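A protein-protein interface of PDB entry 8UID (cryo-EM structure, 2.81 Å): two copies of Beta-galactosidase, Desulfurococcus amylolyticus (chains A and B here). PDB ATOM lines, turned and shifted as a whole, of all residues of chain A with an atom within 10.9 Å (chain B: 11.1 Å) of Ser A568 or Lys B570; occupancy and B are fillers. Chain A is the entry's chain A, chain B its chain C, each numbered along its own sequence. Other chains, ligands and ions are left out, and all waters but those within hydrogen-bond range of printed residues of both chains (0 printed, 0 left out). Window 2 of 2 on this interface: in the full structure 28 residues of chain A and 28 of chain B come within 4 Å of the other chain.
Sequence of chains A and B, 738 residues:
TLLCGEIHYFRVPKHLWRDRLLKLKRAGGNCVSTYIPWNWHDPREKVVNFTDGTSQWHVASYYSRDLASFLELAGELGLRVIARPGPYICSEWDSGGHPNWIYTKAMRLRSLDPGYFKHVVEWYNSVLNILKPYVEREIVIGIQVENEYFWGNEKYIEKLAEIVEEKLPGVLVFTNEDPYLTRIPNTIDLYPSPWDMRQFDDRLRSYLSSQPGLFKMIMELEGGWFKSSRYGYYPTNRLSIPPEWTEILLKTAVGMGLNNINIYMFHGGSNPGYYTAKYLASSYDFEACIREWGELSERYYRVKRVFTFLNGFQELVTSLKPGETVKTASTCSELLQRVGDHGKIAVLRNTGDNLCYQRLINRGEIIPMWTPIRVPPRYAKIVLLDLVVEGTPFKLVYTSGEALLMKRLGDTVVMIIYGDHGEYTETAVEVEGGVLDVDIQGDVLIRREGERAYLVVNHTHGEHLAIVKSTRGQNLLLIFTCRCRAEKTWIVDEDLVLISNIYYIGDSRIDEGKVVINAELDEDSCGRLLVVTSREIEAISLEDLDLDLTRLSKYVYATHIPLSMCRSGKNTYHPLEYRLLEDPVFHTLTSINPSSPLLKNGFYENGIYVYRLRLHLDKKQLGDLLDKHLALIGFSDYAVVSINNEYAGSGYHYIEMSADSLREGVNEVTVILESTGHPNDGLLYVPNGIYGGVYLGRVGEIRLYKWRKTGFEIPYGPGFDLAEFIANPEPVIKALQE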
ATOM      1  N   LEU A 521      15.935  19.340  24.635  1.00  0.00           N
ATOM      2  CA  LEU A 521      17.296  19.011  25.018  1.00  0.00           C
ATOM      3  C   LEU A 521      18.225  19.072  23.807  1.00  0.00           C
ATOM      4  O   LEU A 521      18.019  18.365  22.825  1.00  0.00           O
ATOM      5  CB  LEU A 521      17.341  17.609  25.644  1.00  0.00           C
ATOM      6  CG  LEU A 521      16.771  17.459  27.064  1.00  0.00           C
ATOM      7  CD1 LEU A 521      15.251  17.518  27.129  1.00  0.00           C
ATOM      8  CD2 LEU A 521      17.199  16.098  27.599  1.00  0.00           C
ATOM      9  N   ASP A 522      19.288  19.854  23.917  1.00  0.00           N
ATOM     10  CA  ASP A 522      20.455  19.802  23.045  1.00  0.00           C
ATOM     11  C   ASP A 522      21.558  18.916  23.655  1.00  0.00           C
ATOM     12  O   ASP A 522      21.397  18.342  24.729  1.00  0.00           O
ATOM     13  CB  ASP A 522      20.937  21.225  22.735  1.00  0.00           C
ATOM     14  CG  ASP A 522      21.686  21.945  23.858  1.00  0.00           C
ATOM     15  OD1 ASP A 522      21.776  21.407  24.980  1.00  0.00           O
ATOM     16  OD2 ASP A 522      22.203  23.052  23.581  1.00  0.00           O
ATOM     17  N   GLU A 523      22.702  18.774  22.992  1.00  0.00           N
ATOM     18  CA  GLU A 523      23.794  17.929  23.477  1.00  0.00           C
ATOM     19  C   GLU A 523      24.510  18.457  24.739  1.00  0.00           C
ATOM     20  O   GLU A 523      25.397  17.785  25.263  1.00  0.00           O
ATOM     21  CB  GLU A 523      24.774  17.633  22.335  1.00  0.00           C
ATOM     22  CG  GLU A 523      25.421  18.873  21.716  1.00  0.00           C
ATOM     23  CD  GLU A 523      24.687  19.301  20.440  1.00  0.00           C
ATOM     24  OE1 GLU A 523      25.191  18.998  19.334  1.00  0.00           O
ATOM     25  OE2 GLU A 523      23.607  19.921  20.547  1.00  0.00           O
ATOM     26  N   ASP A 524      24.141  19.625  25.261  1.00  0.00           N
ATOM     27  CA  ASP A 524      24.611  20.141  26.548  1.00  0.00           C
ATOM     28  C   ASP A 524      23.593  19.917  27.677  1.00  0.00           C
ATOM     29  O   ASP A 524      23.911  20.126  28.844  1.00  0.00           O
ATOM     30  CB  ASP A 524      24.940  21.637  26.439  1.00  0.00           C
ATOM     31  CG  ASP A 524      26.018  21.999  25.410  1.00  0.00           C
ATOM     32  OD1 ASP A 524      26.836  21.135  25.025  1.00  0.00           O
ATOM     33  OD2 ASP A 524      26.098  23.191  25.032  1.00  0.00           O
ATOM     34  N   SER A 525      22.365  19.509  27.352  1.00  0.00           N
ATOM     35  CA  SER A 525      21.205  19.597  28.241  1.00  0.00           C
ATOM     36  C   SER A 525      21.110  18.568  29.363  1.00  0.00           C
ATOM     37  O   SER A 525      20.302  18.728  30.272  1.00  0.00           O
ATOM     38  CB  SER A 525      19.951  19.533  27.391  1.00  0.00           C
ATOM     39  OG  SER A 525      19.833  20.717  26.637  1.00  0.00           O
ATOM     40  N   CYS A 526      21.911  17.514  29.317  1.00  0.00           N
ATOM     41  CA  CYS A 526      21.972  16.488  30.354  1.00  0.00           C
ATOM     42  C   CYS A 526      22.830  16.918  31.551  1.00  0.00           C
ATOM     43  O   CYS A 526      23.451  17.977  31.543  1.00  0.00           O
ATOM     44  CB  CYS A 526      22.461  15.203  29.698  1.00  0.00           C
ATOM     45  SG  CYS A 526      21.197  14.715  28.499  1.00  0.00           S
ATOM     46  N   PRO A 562      20.303  11.638  32.355  1.00  0.00           N
ATOM     47  CA  PRO A 562      21.507  10.916  31.958  1.00  0.00           C
ATOM     48  C   PRO A 562      22.154  11.493  30.703  1.00  0.00           C
ATOM     49  O   PRO A 562      21.445  11.883  29.778  1.00  0.00           O
ATOM     50  CB  PRO A 562      21.058   9.472  31.745  1.00  0.00           C
ATOM     51  CG  PRO A 562      19.842   9.335  32.650  1.00  0.00           C
ATOM     52  CD  PRO A 562      19.201  10.707  32.542  1.00  0.00           C
ATOM     53  N   LEU A 563      23.487  11.501  30.605  1.00  0.00           N
ATOM     54  CA  LEU A 563      24.199  11.971  29.403  1.00  0.00           C
ATOM     55  C   LEU A 563      23.897  11.124  28.152  1.00  0.00           C
ATOM     56  O   LEU A 563      24.107  11.584  27.033  1.00  0.00           O
ATOM     57  CB  LEU A 563      25.716  12.052  29.671  1.00  0.00           C
ATOM     58  CG  LEU A 563      26.184  13.425  30.182  1.00  0.00           C
ATOM     59  CD1 LEU A 563      25.763  13.701  31.626  1.00  0.00           C
ATOM     60  CD2 LEU A 563      27.703  13.531  30.075  1.00  0.00           C
ATOM     61  N   SER A 564      23.350   9.920  28.316  1.00  0.00           N
ATOM     62  CA  SER A 564      22.830   9.087  27.230  1.00  0.00           C
ATOM     63  C   SER A 564      21.508   9.586  26.615  1.00  0.00           C
ATOM     64  O   SER A 564      21.153   9.141  25.524  1.00  0.00           O
ATOM     65  CB  SER A 564      22.658   7.658  27.753  1.00  0.00           C
ATOM     66  OG  SER A 564      21.801   7.621  28.879  1.00  0.00           O
ATOM     67  N   MET A 565      20.766  10.496  27.265  1.00  0.00           N
ATOM     68  CA  MET A 565      19.486  11.008  26.749  1.00  0.00           C
ATOM     69  C   MET A 565      19.660  11.940  25.545  1.00  0.00           C
ATOM     70  O   MET A 565      18.980  11.764  24.533  1.00  0.00           O
ATOM     71  CB  MET A 565      18.686  11.751  27.832  1.00  0.00           C
ATOM     72  CG  MET A 565      18.233  10.876  28.999  1.00  0.00           C
ATOM     73  SD  MET A 565      17.078   9.547  28.574  1.00  0.00           S
ATOM     74  CE  MET A 565      18.221   8.144  28.434  1.00  0.00           C
ATOM     75  N   CYS A 566      20.529  12.949  25.643  1.00  0.00           N
ATOM     76  CA  CYS A 566      20.723  13.916  24.561  1.00  0.00           C
ATOM     77  C   CYS A 566      21.479  13.309  23.369  1.00  0.00           C
ATOM     78  O   CYS A 566      22.257  12.362  23.512  1.00  0.00           O
ATOM     79  CB  CYS A 566      21.400  15.190  25.085  1.00  0.00           C
ATOM     80  SG  CYS A 566      23.113  14.896  25.620  1.00  0.00           S
ATOM     81  N   ARG A 567      21.254  13.864  22.174  1.00  0.00           N
ATOM     82  CA  ARG A 567      21.898  13.479  20.907  1.00  0.00           C
ATOM     83  C   ARG A 567      22.430  14.719  20.193  1.00  0.00           C
ATOM     84  O   ARG A 567      21.824  15.786  20.265  1.00  0.00           O
ATOM     85  CB  ARG A 567      20.898  12.731  20.000  1.00  0.00           C
ATOM     86  CG  ARG A 567      20.335  11.398  20.526  1.00  0.00           C
ATOM     87  CD  ARG A 567      21.334  10.231  20.499  1.00  0.00           C
ATOM     88  NE  ARG A 567      22.350  10.353  21.556  1.00  0.00           N
ATOM     89  CZ  ARG A 567      23.511   9.739  21.647  1.00  0.00           C
ATOM     90  NH1 ARG A 567      23.903   8.841  20.791  1.00  0.00           N
ATOM     91  NH2 ARG A 567      24.310  10.045  22.624  1.00  0.00           N
ATOM     92  N   SER A 568      23.537  14.564  19.473  1.00  0.00           N
ATOM     93  CA  SER A 568      24.054  15.562  18.533  1.00  0.00           C
ATOM     94  C   SER A 568      23.817  15.080  17.101  1.00  0.00           C
ATOM     95  O   SER A 568      24.191  13.958  16.751  1.00  0.00           O
ATOM     96  CB  SER A 568      25.541  15.809  18.792  1.00  0.00           C
ATOM     97  OG  SER A 568      26.002  16.889  18.006  1.00  0.00           O
ATOM     98  N   GLY A 569      23.172  15.900  16.274  1.00  0.00           N
ATOM     99  CA  GLY A 569      22.781  15.546  14.910  1.00  0.00           C
ATOM    100  C   GLY A 569      22.407  16.775  14.090  1.00  0.00           C
ATOM    101  O   GLY A 569      21.921  17.764  14.640  1.00  0.00           O
ATOM    102  N   LYS A 570      22.684  16.727  12.784  1.00  0.00           N
ATOM    103  CA  LYS A 570      22.629  17.876  11.864  1.00  0.00           C
ATOM    104  C   LYS A 570      22.533  17.391  10.410  1.00  0.00           C
ATOM    105  O   LYS A 570      23.403  17.660   9.587  1.00  0.00           O
ATOM    106  CB  LYS A 570      23.866  18.753  12.146  1.00  0.00           C
ATOM    107  CG  LYS A 570      23.777  20.169  11.563  1.00  0.00           C
ATOM    108  CD  LYS A 570      25.064  20.944  11.865  1.00  0.00           C
ATOM    109  CE  LYS A 570      24.986  22.366  11.300  1.00  0.00           C
ATOM    110  NZ  LYS A 570      26.228  23.128  11.581  1.00  0.00           N
ATOM    111  N   ASN A 571      21.524  16.572  10.120  1.00  0.00           N
ATOM    112  CA  ASN A 571      21.344  15.873   8.841  1.00  0.00           C
ATOM    113  C   ASN A 571      21.126  16.822   7.643  1.00  0.00           C
ATOM    114  O   ASN A 571      20.595  17.921   7.794  1.00  0.00           O
ATOM    115  CB  ASN A 571      20.162  14.896   8.962  1.00  0.00           C
ATOM    116  CG  ASN A 571      20.288  13.861  10.073  1.00  0.00           C
ATOM    117  OD1 ASN A 571      20.466  14.177  11.241  1.00  0.00           O
ATOM    118  ND2 ASN A 571      20.196  12.593   9.753  1.00  0.00           N
ATOM    119  N   THR A 572      21.473  16.379   6.432  1.00  0.00           N
ATOM    120  CA  THR A 572      21.163  17.076   5.174  1.00  0.00           C
ATOM    121  C   THR A 572      20.451  16.160   4.190  1.00  0.00           C
ATOM    122  O   THR A 572      20.706  14.960   4.130  1.00  0.00           O
ATOM    123  CB  THR A 572      22.377  17.740   4.501  1.00  0.00           C
ATOM    124  OG1 THR A 572      23.302  16.800   4.004  1.00  0.00           O
ATOM    125  CG2 THR A 572      23.151  18.643   5.453  1.00  0.00           C
ATOM    126  N   TYR B 234      35.924  31.138  28.588  1.00  0.00           N
ATOM    127  CA  TYR B 234      35.965  29.988  27.665  1.00  0.00           C
ATOM    128  C   TYR B 234      36.880  30.175  26.444  1.00  0.00           C
ATOM    129  O   TYR B 234      37.779  29.340  26.273  1.00  0.00           O
ATOM    130  CB  TYR B 234      34.561  29.485  27.259  1.00  0.00           C
ATOM    131  CG  TYR B 234      34.508  28.851  25.872  1.00  0.00           C
ATOM    132  CD1 TYR B 234      35.375  27.787  25.546  1.00  0.00           C
ATOM    133  CD2 TYR B 234      33.729  29.443  24.861  1.00  0.00           C
ATOM    134  CE1 TYR B 234      35.540  27.386  24.212  1.00  0.00           C
ATOM    135  CE2 TYR B 234      33.885  29.040  23.521  1.00  0.00           C
ATOM    136  CZ  TYR B 234      34.814  28.029  23.191  1.00  0.00           C
ATOM    137  OH  TYR B 234      35.027  27.682  21.894  1.00  0.00           O
ATOM    138  N   TRP B 293      42.542  21.506  18.276  1.00  0.00           N
ATOM    139  CA  TRP B 293      42.114  20.279  17.616  1.00  0.00           C
ATOM    140  C   TRP B 293      42.353  20.247  16.094  1.00  0.00           C
ATOM    141  O   TRP B 293      42.021  19.258  15.455  1.00  0.00           O
ATOM    142  CB  TRP B 293      40.648  20.029  17.990  1.00  0.00           C
ATOM    143  CG  TRP B 293      39.721  21.192  17.863  1.00  0.00           C
ATOM    144  CD1 TRP B 293      38.980  21.512  16.781  1.00  0.00           C
ATOM    145  CD2 TRP B 293      39.460  22.224  18.852  1.00  0.00           C
ATOM    146  NE1 TRP B 293      38.276  22.670  17.037  1.00  0.00           N
ATOM    147  CE2 TRP B 293      38.535  23.152  18.300  1.00  0.00           C
ATOM    148  CE3 TRP B 293      39.922  22.471  20.161  1.00  0.00           C
ATOM    149  CZ2 TRP B 293      38.090  24.274  19.009  1.00  0.00           C
ATOM    150  CZ3 TRP B 293      39.495  23.603  20.876  1.00  0.00           C
ATOM    151  CH2 TRP B 293      38.579  24.499  20.303  1.00  0.00           C
ATOM    152  N   GLU B 295      41.290  22.726  13.715  1.00  0.00           N
ATOM    153  CA  GLU B 295      40.262  23.419  12.937  1.00  0.00           C
ATOM    154  C   GLU B 295      40.748  24.750  12.358  1.00  0.00           C
ATOM    155  O   GLU B 295      41.228  25.603  13.091  1.00  0.00           O
ATOM    156  CB  GLU B 295      39.070  23.661  13.847  1.00  0.00           C
ATOM    157  CG  GLU B 295      37.820  24.226  13.183  1.00  0.00           C
ATOM    158  CD  GLU B 295      36.895  24.806  14.257  1.00  0.00           C
ATOM    159  OE1 GLU B 295      36.596  24.098  15.243  1.00  0.00           O
ATOM    160  OE2 GLU B 295      36.483  25.979  14.124  1.00  0.00           O
ATOM    161  N   ASP B 522      34.555  19.988   4.192  1.00  0.00           N
ATOM    162  CA  ASP B 522      33.430  20.188   5.098  1.00  0.00           C
ATOM    163  C   ASP B 522      32.109  20.313   4.315  1.00  0.00           C
ATOM    164  O   ASP B 522      32.080  20.226   3.090  1.00  0.00           O
ATOM    165  CB  ASP B 522      33.701  21.394   6.006  1.00  0.00           C
ATOM    166  CG  ASP B 522      33.554  22.774   5.361  1.00  0.00           C
ATOM    167  OD1 ASP B 522      33.333  22.857   4.135  1.00  0.00           O
ATOM    168  OD2 ASP B 522      33.639  23.769   6.116  1.00  0.00           O
ATOM    169  N   GLU B 523      30.983  20.518   4.992  1.00  0.00           N
ATOM    170  CA  GLU B 523      29.677  20.618   4.337  1.00  0.00           C
ATOM    171  C   GLU B 523      29.476  21.891   3.485  1.00  0.00           C
ATOM    172  O   GLU B 523      28.438  22.037   2.842  1.00  0.00           O
ATOM    173  CB  GLU B 523      28.559  20.429   5.369  1.00  0.00           C
ATOM    174  CG  GLU B 523      28.561  21.456   6.506  1.00  0.00           C
ATOM    175  CD  GLU B 523      29.258  20.899   7.752  1.00  0.00           C
ATOM    176  OE1 GLU B 523      28.547  20.478   8.693  1.00  0.00           O
ATOM    177  OE2 GLU B 523      30.507  20.870   7.778  1.00  0.00           O
ATOM    178  N   ARG B 567      29.645  15.707   3.598  1.00  0.00           N
ATOM    179  CA  ARG B 567      28.754  15.230   4.669  1.00  0.00           C
ATOM    180  C   ARG B 567      28.843  16.159   5.877  1.00  0.00           C
ATOM    181  O   ARG B 567      29.910  16.697   6.170  1.00  0.00           O
ATOM    182  CB  ARG B 567      29.127  13.788   5.079  1.00  0.00           C
ATOM    183  CG  ARG B 567      28.995  12.697   4.001  1.00  0.00           C
ATOM    184  CD  ARG B 567      27.548  12.301   3.672  1.00  0.00           C
ATOM    185  NE  ARG B 567      26.861  13.331   2.877  1.00  0.00           N
ATOM    186  CZ  ARG B 567      25.568  13.484   2.682  1.00  0.00           C
ATOM    187  NH1 ARG B 567      24.681  12.653   3.145  1.00  0.00           N
ATOM    188  NH2 ARG B 567      25.152  14.515   2.009  1.00  0.00           N
ATOM    189  N   SER B 568      27.736  16.310   6.597  1.00  0.00           N
ATOM    190  CA  SER B 568      27.690  16.958   7.911  1.00  0.00           C
ATOM    191  C   SER B 568      27.484  15.895   8.991  1.00  0.00           C
ATOM    192  O   SER B 568      26.557  15.087   8.903  1.00  0.00           O
ATOM    193  CB  SER B 568      26.573  18.003   7.944  1.00  0.00           C
ATOM    194  OG  SER B 568      26.634  18.745   9.146  1.00  0.00           O
ATOM    195  N   GLY B 569      28.355  15.863   9.998  1.00  0.00           N
ATOM    196  CA  GLY B 569      28.354  14.848  11.049  1.00  0.00           C
ATOM    197  C   GLY B 569      29.201  15.269  12.245  1.00  0.00           C
ATOM    198  O   GLY B 569      30.180  15.998  12.087  1.00  0.00           O
ATOM    199  N   LYS B 570      28.791  14.848  13.445  1.00  0.00           N
ATOM    200  CA  LYS B 570      29.312  15.327  14.735  1.00  0.00           C
ATOM    201  C   LYS B 570      28.983  14.325  15.851  1.00  0.00           C
ATOM    202  O   LYS B 570      28.279  14.640  16.807  1.00  0.00           O
ATOM    203  CB  LYS B 570      28.730  16.736  14.973  1.00  0.00           C
ATOM    204  CG  LYS B 570      29.455  17.538  16.060  1.00  0.00           C
ATOM    205  CD  LYS B 570      28.783  18.902  16.246  1.00  0.00           C
ATOM    206  CE  LYS B 570      29.503  19.720  17.322  1.00  0.00           C
ATOM    207  NZ  LYS B 570      28.858  21.044  17.515  1.00  0.00           N
ATOM    208  N   ASN B 571      29.399  13.074  15.669  1.00  0.00           N
ATOM    209  CA  ASN B 571      29.051  11.935  16.530  1.00  0.00           C
ATOM    210  C   ASN B 571      29.581  12.069  17.975  1.00  0.00           C
ATOM    211  O   ASN B 571      30.608  12.700  18.218  1.00  0.00           O
ATOM    212  CB  ASN B 571      29.582  10.639  15.892  1.00  0.00           C
ATOM    213  CG  ASN B 571      29.079  10.359  14.481  1.00  0.00           C
ATOM    214  OD1 ASN B 571      29.220  11.160  13.568  1.00  0.00           O
ATOM    215  ND2 ASN B 571      28.480   9.216  14.254  1.00  0.00           N
ATOM    216  N   THR B 572      28.920  11.421  18.938  1.00  0.00           N
ATOM    217  CA  THR B 572      29.394  11.290  20.325  1.00  0.00           C
ATOM    218  C   THR B 572      29.426   9.836  20.769  1.00  0.00           C
ATOM    219  O   THR B 572      28.594   9.024  20.370  1.00  0.00           O
ATOM    220  CB  THR B 572      28.613  12.142  21.343  1.00  0.00           C
ATOM    221  OG1 THR B 572      27.290  11.691  21.523  1.00  0.00           O
ATOM    222  CG2 THR B 572      28.518  13.604  20.929  1.00  0.00           C
ATOM    223  N   TYR B 573      30.389   9.513  21.621  1.00  0.00           N
ATOM    224  CA  TYR B 573      30.694   8.171  22.088  1.00  0.00           C
ATOM    225  C   TYR B 573      30.726   8.180  23.609  1.00  0.00           C
ATOM    226  O   TYR B 573      31.323   9.066  24.213  1.00  0.00           O
ATOM    227  CB  TYR B 573      32.029   7.700  21.495  1.00  0.00           C
ATOM    228  CG  TYR B 573      32.178   7.909  19.999  1.00  0.00           C
ATOM    229  CD1 TYR B 573      32.593   9.157  19.492  1.00  0.00           C
ATOM    230  CD2 TYR B 573      31.848   6.871  19.112  1.00  0.00           C
ATOM    231  CE1 TYR B 573      32.614   9.386  18.107  1.00  0.00           C
ATOM    232  CE2 TYR B 573      31.903   7.086  17.725  1.00  0.00           C
ATOM    233  CZ  TYR B 573      32.273   8.346  17.221  1.00  0.00           C
ATOM    234  OH  TYR B 573      32.273   8.554  15.881  1.00  0.00           O
ATOM    235  N   HIS B 574      30.089   7.198  24.237  1.00  0.00           N
ATOM    236  CA  HIS B 574      29.859   7.139  25.681  1.00  0.00           C
ATOM    237  C   HIS B 574      30.491   5.876  26.275  1.00  0.00           C
ATOM    238  O   HIS B 574      30.644   4.888  25.557  1.00  0.00           O
ATOM    239  CB  HIS B 574      28.353   7.176  25.951  1.00  0.00           C
ATOM    240  CG  HIS B 574      27.672   8.416  25.442  1.00  0.00           C
ATOM    241  ND1 HIS B 574      27.633   9.637  26.069  1.00  0.00           N
ATOM    242  CD2 HIS B 574      27.066   8.569  24.227  1.00  0.00           C
ATOM    243  CE1 HIS B 574      27.018  10.505  25.257  1.00  0.00           C
ATOM    244  NE2 HIS B 574      26.663   9.904  24.109  1.00  0.00           N
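O of Lys B570 is in hydrogen-bond range of OG of Ser A568 (3.4 Å).
The guanidinium group (NH2) of Arg A567 is in hydrogen-bond range of a ring nitrogen (NE2) of His B574 (2.8 Å).
The backbone carbonyl oxygen (O) of Lys A570 sits at hydrogen-bond distance from the side-chain hydroxyl (OG) of Ser B568 (3.4 Å).
OE1 of Glu A523 is in hydrogen-bond range of OG of Ser A568 (2.6 Å).
The side-chain hydroxyl (OG) of Ser B568 sits at hydrogen-bond distance from the side-chain carboxylate (OE1) of Glu B523, 2.6 Å away.
The side-chain hydroxyl (OG1) of Thr B572 sits at hydrogen-bond distance from a ring nitrogen (NE2) of His B574.
O of Leu A563 lies within hydrogen-bond range of SG of Cys A566, 3.7 Å away.
Among the printed residues, pairs that only touch across the chains: Thr A572 with Arg B567, Leu A563 with His B574 and Arg A567 with Thr B572.
Lys B570 touches just one residue of chain A: Ser A568.
No residue of chain B comes within 4 Å of Glu A523.
Of chain B, only Thr B572 and His B574 come within 4 Å of Arg A567.
No residue of chain A comes within 4 Å of Gly B569.
Of the printed residues of chain A, Ser B568 touches Lys A570 (3.4 Å).
Printed residues of chain B within 4 Å of Thr A572: Arg B567 (3.6 Å).
Of the printed residues of chain A, Arg B567 touches Thr A572.
The nearest printed residue of chain A that does not touch His B574 is Ser A564 (4.8 Å).
Of the 17 printed residues of chain A, 5 touch a printed residue of chain B.
Printed residues of chain B that touch a printed residue of chain A: Arg B567, Ser B568, Lys B570, Thr B572 and His B574.
Among the printed residues, 6 pairs touch across the chains.
Among the printed residues, no Asp or Glu carboxylate lies within 4 Å of a Lys or Arg side-chain nitrogen of the other chain.
Arg A567 touches Thr B572, and with the chains exchanged Thr A572 touches Arg B567.
Ser A568 touches Lys B570, and with the chains exchanged Lys A570 touches Ser B568.
8 positions are printed for both chains.
Of the 6 pairs that touch across the chains among the printed residues, 4 have their exchanged pair printed and touching as well.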
